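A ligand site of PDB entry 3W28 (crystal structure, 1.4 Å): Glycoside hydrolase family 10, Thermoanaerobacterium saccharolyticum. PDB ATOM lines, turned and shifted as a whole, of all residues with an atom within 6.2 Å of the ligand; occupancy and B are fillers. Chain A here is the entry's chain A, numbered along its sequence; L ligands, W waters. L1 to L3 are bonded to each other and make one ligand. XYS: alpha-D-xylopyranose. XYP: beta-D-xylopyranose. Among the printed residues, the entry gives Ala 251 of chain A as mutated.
The backbone carbonyl oxygen (O) of Glu 48 lies within hydrogen-bond range of the side-chain amino group (NZ) of Lys 52 (3.0 Å).
ND1 of His 223 lies close to O of Ala 251, at 3.1 Å.
ND1 of His 85 lies within hydrogen-bond range of OD2 of Asp 142, at 2.8 Å.
The side-chain amide oxygen (OD1) of Asn 145 sits close to the side-chain amide oxygen (OE1) of Gln 221 (3.4 Å).
The indole nitrogen (NE1) of Trp 89 sits close to the side-chain amide nitrogen (ND2) of Asn 145.
The side-chain amide oxygen (OD1) of Asn 145 sits at hydrogen-bond distance from the side-chain amide nitrogen (ND2) of Asn 187, at 2.9 Å.
The side-chain amide nitrogen of Gln 92 is in hydrogen-bond range of the side-chain amide oxygen of Asn 49, at 3.0 Å.
The side-chain carboxylate (OE2) of Glu 146 sits close to the side-chain amide oxygen (OE1) of Gln 221, 3.0 Å away.
CH2 of Trp 89 touches O3 of XYS L1 (3.4 Å).
OE2 of Glu 146 touches C1 of XYS L1, at 3.7 Å.
CB of Ala 251 touches O1 of XYS L1, at 3.6 Å.
CB of Trp 300 touches O2 of XYP L2, 3.3 Å away.
Within 4 Å of the ligand: Glu 48, Asn 49, Lys 52, His 85, Trp 89, Gln 92, Asn 145, Glu 146, Gln 221, His 223, Ala 251, Trp 292 and Trp 300.
Water W6 lies within hydrogen-bond range of O4 of XYP L3 and OE2 of Glu 54.
Water W3 bridges an oxygen (O5) of XYP L3 and the side-chain amide nitrogen (ND2) of Asn 49.
Water W4 bridges an oxygen (O5) of XYS L1 (2.7 Å) and the side-chain carboxylate of Glu 146 (3.0 Å).
Water W5 lies within hydrogen-bond range of NE2 of Gln 221 (2.9 Å), O5 of XYS L1 (3.3 Å) and OE2 of Glu 146 (3.5 Å).
The side-chain carboxylate (OE2) of Glu 48 is in hydrogen-bond range of an oxygen (O2) of XYP L2 (2.7 Å).
A ring nitrogen (NE2) of His 223 lies within hydrogen-bond range of an oxygen (O1) of XYS L1 (2.7 Å).
O3 of XYS L1 sits at hydrogen-bond distance from NE2 of His 85 (2.8 Å).
The indole nitrogen (NE1) of Trp 292 is in hydrogen-bond range of an oxygen (O2) of XYP L2 (2.8 Å).
The side-chain amino group (NZ) of Lys 52 is in hydrogen-bond range of an oxygen (O3) of XYS L1.
An oxygen (O2) of XYS L1 lies within hydrogen-bond range of the side-chain amide nitrogen (ND2) of Asn 145, at 3.0 Å.
An oxygen (O3) of XYP L2 lies within hydrogen-bond range of the side-chain amide nitrogen (ND2) of Asn 49 (3.0 Å).
O5 of XYP L2 lies close to OE1 of Gln 92, at 3.2 Å.
The side-chain amide oxygen (OE1) of Gln 221 lies within hydrogen-bond range of an oxygen (O2) of XYS L1 (3.2 Å).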
ATOM      1  N   GLU A  48      -3.562  31.032   4.186  1.00  0.00           N
ATOM      2  CA  GLU A  48      -3.514  31.189   5.629  1.00  0.00           C
ATOM      3  C   GLU A  48      -4.549  32.217   6.106  1.00  0.00           C
ATOM      4  O   GLU A  48      -5.131  32.058   7.190  1.00  0.00           O
ATOM      5  CB  GLU A  48      -2.096  31.624   6.049  1.00  0.00           C
ATOM      6  CG  GLU A  48      -1.890  31.634   7.570  1.00  0.00           C
ATOM      7  CD  GLU A  48      -0.488  31.978   7.992  1.00  0.00           C
ATOM      8  OE1 GLU A  48       0.320  32.409   7.139  1.00  0.00           O
ATOM      9  OE2 GLU A  48      -0.220  31.835   9.204  1.00  0.00           O
ATOM     10  N   ASN A  49      -4.760  33.246   5.293  1.00  0.00           N
ATOM     11  CA  ASN A  49      -5.680  34.329   5.646  1.00  0.00           C
ATOM     12  C   ASN A  49      -6.504  34.884   4.486  1.00  0.00           C
ATOM     13  O   ASN A  49      -7.597  35.410   4.709  1.00  0.00           O
ATOM     14  CB  ASN A  49      -4.899  35.504   6.226  1.00  0.00           C
ATOM     15  CG  ASN A  49      -4.367  35.203   7.599  1.00  0.00           C
ATOM     16  OD1 ASN A  49      -5.142  34.977   8.546  1.00  0.00           O
ATOM     17  ND2 ASN A  49      -3.038  35.153   7.723  1.00  0.00           N
ATOM     18  N   LYS A  52     -10.430  34.135   4.145  1.00  0.00           N
ATOM     19  CA  LYS A  52     -11.312  34.327   5.297  1.00  0.00           C
ATOM     20  C   LYS A  52     -12.367  35.385   4.972  1.00  0.00           C
ATOM     21  O   LYS A  52     -12.200  36.190   4.081  1.00  0.00           O
ATOM     22  CB  LYS A  52     -10.496  34.706   6.539  1.00  0.00           C
ATOM     23  CG  LYS A  52      -9.751  33.489   7.053  1.00  0.00           C
ATOM     24  CD  LYS A  52      -8.683  33.833   8.100  1.00  0.00           C
ATOM     25  CE  LYS A  52      -7.974  32.563   8.624  1.00  0.00           C
ATOM     26  NZ  LYS A  52      -6.802  32.880   9.512  1.00  0.00           N
ATOM     27  N   GLU A  54     -13.285  38.326   6.270  1.00  0.00           N
ATOM     28  CA  GLU A  54     -12.860  39.740   6.208  1.00  0.00           C
ATOM     29  C   GLU A  54     -11.935  40.002   5.021  1.00  0.00           C
ATOM     30  O   GLU A  54     -11.844  41.131   4.524  1.00  0.00           O
ATOM     31  CB  GLU A  54     -12.137  40.144   7.515  1.00  0.00           C
ATOM     32  CG  GLU A  54     -10.672  39.611   7.581  1.00  0.00           C
ATOM     33  CD  GLU A  54      -9.914  39.958   8.885  1.00  0.00           C
ATOM     34  OE1 GLU A  54     -10.518  40.516   9.806  1.00  0.00           O
ATOM     35  OE2 GLU A  54      -8.706  39.627   8.951  1.00  0.00           O
ATOM     36  N   HIS A  85     -10.205  27.983   2.786  1.00  0.00           N
ATOM     37  CA  HIS A  85     -10.359  28.265   4.218  1.00  0.00           C
ATOM     38  C   HIS A  85     -10.691  29.758   4.346  1.00  0.00           C
ATOM     39  O   HIS A  85      -9.844  30.574   3.995  1.00  0.00           O
ATOM     40  CB  HIS A  85      -9.028  27.937   4.913  1.00  0.00           C
ATOM     41  CG  HIS A  85      -9.039  28.221   6.387  1.00  0.00           C
ATOM     42  ND1 HIS A  85      -9.661  27.383   7.297  1.00  0.00           N
ATOM     43  CD2 HIS A  85      -8.531  29.247   7.096  1.00  0.00           C
ATOM     44  CE1 HIS A  85      -9.519  27.903   8.519  1.00  0.00           C
ATOM     45  NE2 HIS A  85      -8.838  29.024   8.419  1.00  0.00           N
ATOM     46  N   THR A  86     -11.870  30.173   4.838  1.00  0.00           N
ATOM     47  CA  THR A  86     -12.984  29.350   5.326  1.00  0.00           C
ATOM     48  C   THR A  86     -14.239  30.235   5.118  1.00  0.00           C
ATOM     49  O   THR A  86     -14.151  31.466   5.160  1.00  0.00           O
ATOM     50  CB  THR A  86     -12.802  29.017   6.844  1.00  0.00           C
ATOM     51  OG1 THR A  86     -13.978  28.369   7.341  1.00  0.00           O
ATOM     52  CG2 THR A  86     -12.560  30.277   7.677  1.00  0.00           C
ATOM     53  N   TRP A  89     -16.617  31.830  10.214  1.00  0.00           N
ATOM     54  CA  TRP A  89     -15.791  31.768  11.422  1.00  0.00           C
ATOM     55  C   TRP A  89     -16.265  32.937  12.300  1.00  0.00           C
ATOM     56  O   TRP A  89     -16.965  33.837  11.816  1.00  0.00           O
ATOM     57  CB  TRP A  89     -14.298  31.930  11.035  1.00  0.00           C
ATOM     58  CG  TRP A  89     -13.325  31.565  12.113  1.00  0.00           C
ATOM     59  CD1 TRP A  89     -13.539  30.751  13.182  1.00  0.00           C
ATOM     60  CD2 TRP A  89     -11.937  31.939  12.163  1.00  0.00           C
ATOM     61  NE1 TRP A  89     -12.364  30.583  13.897  1.00  0.00           N
ATOM     62  CE2 TRP A  89     -11.376  31.304  13.297  1.00  0.00           C
ATOM     63  CE3 TRP A  89     -11.118  32.754  11.360  1.00  0.00           C
ATOM     64  CZ2 TRP A  89     -10.029  31.452  13.646  1.00  0.00           C
ATOM     65  CZ3 TRP A  89      -9.776  32.901  11.723  1.00  0.00           C
ATOM     66  CH2 TRP A  89      -9.249  32.244  12.852  1.00  0.00           C
ATOM     67  N   GLN A  92     -11.898  37.070  12.269  1.00  0.00           N
ATOM     68  CA  GLN A  92     -11.591  37.544  10.932  1.00  0.00           C
ATOM     69  C   GLN A  92     -12.833  37.562  10.057  1.00  0.00           C
ATOM     70  O   GLN A  92     -12.816  37.186   8.885  1.00  0.00           O
ATOM     71  CB  GLN A  92     -10.426  36.733  10.336  1.00  0.00           C
ATOM     72  CG  GLN A  92      -9.108  37.127  11.006  1.00  0.00           C
ATOM     73  CD  GLN A  92      -7.945  36.309  10.522  1.00  0.00           C
ATOM     74  OE1 GLN A  92      -7.630  35.262  11.087  1.00  0.00           O
ATOM     75  NE2 GLN A  92      -7.293  36.794   9.441  1.00  0.00           N
ATOM     76  N   ASP A 142     -13.596  24.560   3.998  1.00  0.00           N
ATOM     77  CA  ASP A 142     -13.946  24.527   5.419  1.00  0.00           C
ATOM     78  C   ASP A 142     -15.172  25.459   5.394  1.00  0.00           C
ATOM     79  O   ASP A 142     -15.052  26.700   5.321  1.00  0.00           O
ATOM     80  CB  ASP A 142     -12.849  25.139   6.282  1.00  0.00           C
ATOM     81  CG  ASP A 142     -11.655  24.237   6.431  1.00  0.00           C
ATOM     82  OD1 ASP A 142     -11.838  23.011   6.467  1.00  0.00           O
ATOM     83  OD2 ASP A 142     -10.541  24.793   6.535  1.00  0.00           O
ATOM     84  N   ASN A 145     -15.861  26.930  10.570  1.00  0.00           N
ATOM     85  CA  ASN A 145     -14.626  26.788  11.344  1.00  0.00           C
ATOM     86  C   ASN A 145     -14.879  27.063  12.823  1.00  0.00           C
ATOM     87  O   ASN A 145     -15.503  28.088  13.161  1.00  0.00           O
ATOM     88  CB  ASN A 145     -13.611  27.803  10.792  1.00  0.00           C
ATOM     89  CG  ASN A 145     -12.182  27.496  11.184  1.00  0.00           C
ATOM     90  OD1 ASN A 145     -11.786  26.332  11.207  1.00  0.00           O
ATOM     91  ND2 ASN A 145     -11.398  28.523  11.472  1.00  0.00           N
ATOM     92  N   GLU A 146     -14.449  26.152  13.692  1.00  0.00           N
ATOM     93  CA  GLU A 146     -14.499  26.362  15.145  1.00  0.00           C
ATOM     94  C   GLU A 146     -15.861  26.685  15.707  1.00  0.00           C
ATOM     95  O   GLU A 146     -16.029  27.614  16.521  1.00  0.00           O
ATOM     96  CB  GLU A 146     -13.494  27.467  15.512  1.00  0.00           C
ATOM     97  CG  GLU A 146     -12.045  27.083  15.078  1.00  0.00           C
ATOM     98  CD  GLU A 146     -10.981  28.073  15.480  1.00  0.00           C
ATOM     99  OE1 GLU A 146     -11.329  29.105  16.096  1.00  0.00           O
ATOM    100  OE2 GLU A 146      -9.791  27.823  15.173  1.00  0.00           O
ATOM    101  N   ASN A 187     -14.467  22.223  10.335  1.00  0.00           N
ATOM    102  CA  ASN A 187     -13.076  22.226  10.827  1.00  0.00           C
ATOM    103  C   ASN A 187     -12.950  22.660  12.283  1.00  0.00           C
ATOM    104  O   ASN A 187     -13.681  23.588  12.688  1.00  0.00           O
ATOM    105  CB  ASN A 187     -12.286  23.217   9.939  1.00  0.00           C
ATOM    106  CG  ASN A 187     -10.758  23.082  10.030  1.00  0.00           C
ATOM    107  OD1 ASN A 187     -10.217  21.986   9.925  1.00  0.00           O
ATOM    108  ND2 ASN A 187     -10.064  24.210  10.189  1.00  0.00           N
ATOM    109  N   TYR A 189     -10.233  22.668  16.169  1.00  0.00           N
ATOM    110  CA  TYR A 189      -9.055  22.312  16.960  1.00  0.00           C
ATOM    111  C   TYR A 189      -9.466  21.577  18.207  1.00  0.00           C
ATOM    112  O   TYR A 189     -10.627  21.591  18.614  1.00  0.00           O
ATOM    113  CB  TYR A 189      -8.221  23.565  17.334  1.00  0.00           C
ATOM    114  CG  TYR A 189      -8.924  24.537  18.266  1.00  0.00           C
ATOM    115  CD1 TYR A 189      -8.755  24.471  19.653  1.00  0.00           C
ATOM    116  CD2 TYR A 189      -9.765  25.527  17.754  1.00  0.00           C
ATOM    117  CE1 TYR A 189      -9.403  25.375  20.507  1.00  0.00           C
ATOM    118  CE2 TYR A 189     -10.416  26.431  18.600  1.00  0.00           C
ATOM    119  CZ  TYR A 189     -10.232  26.345  19.970  1.00  0.00           C
ATOM    120  OH  TYR A 189     -10.910  27.256  20.760  1.00  0.00           O
ATOM    121  N   GLN A 221      -7.777  20.415  12.747  1.00  0.00           N
ATOM    122  CA  GLN A 221      -6.662  21.368  12.672  1.00  0.00           C
ATOM    123  C   GLN A 221      -5.281  20.787  13.091  1.00  0.00           C
ATOM    124  O   GLN A 221      -4.270  21.038  12.452  1.00  0.00           O
ATOM    125  CB  GLN A 221      -6.990  22.626  13.498  1.00  0.00           C
ATOM    126  CG  GLN A 221      -8.062  23.495  12.860  1.00  0.00           C
ATOM    127  CD  GLN A 221      -8.431  24.711  13.708  1.00  0.00           C
ATOM    128  OE1 GLN A 221      -9.451  25.392  13.455  1.00  0.00           O
ATOM    129  NE2 GLN A 221      -7.623  25.004  14.693  1.00  0.00           N
ATOM    130  N   HIS A 223      -3.348  21.395  15.907  1.00  0.00           N
ATOM    131  CA  HIS A 223      -2.340  22.286  16.507  1.00  0.00           C
ATOM    132  C   HIS A 223      -1.943  21.531  17.770  1.00  0.00           C
ATOM    133  O   HIS A 223      -2.458  21.758  18.856  1.00  0.00           O
ATOM    134  CB  HIS A 223      -2.961  23.631  16.847  1.00  0.00           C
ATOM    135  CG  HIS A 223      -3.318  24.440  15.628  1.00  0.00           C
ATOM    136  ND1 HIS A 223      -2.371  24.931  14.750  1.00  0.00           N
ATOM    137  CD2 HIS A 223      -4.526  24.811  15.127  1.00  0.00           C
ATOM    138  CE1 HIS A 223      -2.984  25.576  13.763  1.00  0.00           C
ATOM    139  NE2 HIS A 223      -4.279  25.505  13.972  1.00  0.00           N
ATOM    140  N   THR A 250      -5.872  19.492   8.768  1.00  0.00           N
ATOM    141  CA  THR A 250      -5.853  20.782   8.097  1.00  0.00           C
ATOM    142  C   THR A 250      -4.906  21.894   8.503  1.00  0.00           C
ATOM    143  O   THR A 250      -4.686  22.805   7.713  1.00  0.00           O
ATOM    144  CB  THR A 250      -7.265  21.370   8.124  1.00  0.00           C
ATOM    145  OG1 THR A 250      -7.594  21.608   9.509  1.00  0.00           O
ATOM    146  CG2 THR A 250      -8.309  20.407   7.534  1.00  0.00           C
ATOM    147  N   ALA A 251      -4.308  21.835   9.696  1.00  0.00           N
ATOM    148  CA  ALA A 251      -3.453  22.961  10.145  1.00  0.00           C
ATOM    149  C   ALA A 251      -2.357  22.523  11.124  1.00  0.00           C
ATOM    150  O   ALA A 251      -2.078  23.169  12.162  1.00  0.00           O
ATOM    151  CB  ALA A 251      -4.335  23.985  10.827  1.00  0.00           C
ATOM    152  N   TRP A 292       0.461  24.176   8.923  1.00  0.00           N
ATOM    153  CA  TRP A 292       0.032  25.571   9.047  1.00  0.00           C
ATOM    154  C   TRP A 292       1.194  26.539   9.048  1.00  0.00           C
ATOM    155  O   TRP A 292       1.553  27.141  10.062  1.00  0.00           O
ATOM    156  CB  TRP A 292      -0.855  25.754  10.278  1.00  0.00           C
ATOM    157  CG  TRP A 292      -1.808  26.913  10.088  1.00  0.00           C
ATOM    158  CD1 TRP A 292      -1.726  28.146  10.676  1.00  0.00           C
ATOM    159  CD2 TRP A 292      -2.901  26.992   9.162  1.00  0.00           C
ATOM    160  NE1 TRP A 292      -2.681  28.987  10.161  1.00  0.00           N
ATOM    161  CE2 TRP A 292      -3.417  28.309   9.231  1.00  0.00           C
ATOM    162  CE3 TRP A 292      -3.485  26.076   8.262  1.00  0.00           C
ATOM    163  CZ2 TRP A 292      -4.493  28.733   8.432  1.00  0.00           C
ATOM    164  CZ3 TRP A 292      -4.548  26.501   7.467  1.00  0.00           C
ATOM    165  CH2 TRP A 292      -5.033  27.821   7.555  1.00  0.00           C
ATOM    166  N   TRP A 300       2.443  31.240  12.784  1.00  0.00           N
ATOM    167  CA  TRP A 300       1.549  32.123  13.513  1.00  0.00           C
ATOM    168  C   TRP A 300       1.746  32.062  15.030  1.00  0.00           C
ATOM    169  O   TRP A 300       1.244  32.924  15.740  1.00  0.00           O
ATOM    170  CB  TRP A 300       0.083  31.767  13.188  1.00  0.00           C
ATOM    171  CG  TRP A 300      -0.402  30.481  13.792  1.00  0.00           C
ATOM    172  CD1 TRP A 300       0.098  29.220  13.605  1.00  0.00           C
ATOM    173  CD2 TRP A 300      -1.541  30.327  14.664  1.00  0.00           C
ATOM    174  NE1 TRP A 300      -0.657  28.297  14.295  1.00  0.00           N
ATOM    175  CE2 TRP A 300      -1.672  28.949  14.951  1.00  0.00           C
ATOM    176  CE3 TRP A 300      -2.474  31.223  15.222  1.00  0.00           C
ATOM    177  CZ2 TRP A 300      -2.677  28.453  15.779  1.00  0.00           C
ATOM    178  CZ3 TRP A 300      -3.470  30.737  16.046  1.00  0.00           C
ATOM    179  CH2 TRP A 300      -3.566  29.362  16.315  1.00  0.00           C
HETATM  180  C1  XYS L   1      -6.721  27.723  13.131  1.00  0.00           C
HETATM  181  C2  XYS L   1      -7.596  28.611  12.254  1.00  0.00           C
HETATM  182  C3  XYS L   1      -6.740  29.435  11.322  1.00  0.00           C
HETATM  183  C4  XYS L   1      -5.766  30.259  12.165  1.00  0.00           C
HETATM  184  C5  XYS L   1      -4.928  29.286  12.975  1.00  0.00           C
HETATM  185  O1  XYS L   1      -6.017  26.764  12.342  1.00  0.00           O
HETATM  186  O2  XYS L   1      -8.529  27.813  11.502  1.00  0.00           O
HETATM  187  O3  XYS L   1      -7.555  30.331  10.549  1.00  0.00           O
HETATM  188  O4  XYS L   1      -4.936  31.012  11.261  1.00  0.00           O
HETATM  189  O5  XYS L   1      -5.794  28.550  13.851  1.00  0.00           O
HETATM  190  C1  XYP L   2      -4.368  32.151  11.900  1.00  0.00           C
HETATM  191  C2  XYP L   2      -3.309  32.669  10.934  1.00  0.00           C
HETATM  192  C3  XYP L   2      -2.743  33.996  11.431  1.00  0.00           C
HETATM  193  C4  XYP L   2      -3.883  34.961  11.707  1.00  0.00           C
HETATM  194  C5  XYP L   2      -4.874  34.318  12.659  1.00  0.00           C
HETATM  195  O2  XYP L   2      -2.258  31.693  10.913  1.00  0.00           O
HETATM  196  O3  XYP L   2      -1.928  34.554  10.402  1.00  0.00           O
HETATM  197  O4  XYP L   2      -3.325  36.119  12.328  1.00  0.00           O
HETATM  198  O5  XYP L   2      -5.404  33.141  12.047  1.00  0.00           O
HETATM  199  C1  XYP L   3      -4.071  37.301  12.016  1.00  0.00           C
HETATM  200  C2  XYP L   3      -3.647  38.368  12.994  1.00  0.00           C
HETATM  201  C3  XYP L   3      -4.330  39.683  12.644  1.00  0.00           C
HETATM  202  C4  XYP L   3      -4.025  40.024  11.193  1.00  0.00           C
HETATM  203  C5  XYP L   3      -4.444  38.869  10.306  1.00  0.00           C
HETATM  204  O2  XYP L   3      -4.017  37.969  14.324  1.00  0.00           O
HETATM  205  O3  XYP L   3      -3.808  40.724  13.478  1.00  0.00           O
HETATM  206  O4  XYP L   3      -4.769  41.194  10.837  1.00  0.00           O
HETATM  207  O5  XYP L   3      -3.713  37.688  10.681  1.00  0.00           O
HETATM  208  O   HOH W   1      -1.021  41.101  13.062  1.00  0.00           O
HETATM  209  O   HOH W   2      -6.929  26.237   9.790  1.00  0.00           O
HETATM  210  O   HOH W   3      -1.358  37.720   9.294  1.00  0.00           O
HETATM  211  O   HOH W   4      -7.502  29.600  15.733  1.00  0.00           O
HETATM  212  O   HOH W   5      -6.752  26.957  16.627  1.00  0.00           O
HETATM  213  O   HOH W   6      -7.431  40.950  10.930  1.00  0.00           O
HETATM  214  O   HOH W   7       0.305  35.392  11.764  1.00  0.00           O
HETATM  215  O   HOH W   8      -2.560  35.673  15.350  1.00  0.00           O
HETATM  216  O   HOH W   9      -6.963  37.763  14.362  1.00  0.00           O
HETATM  217  O   HOH W  10      -1.110  39.813  15.397  1.00  0.00           O
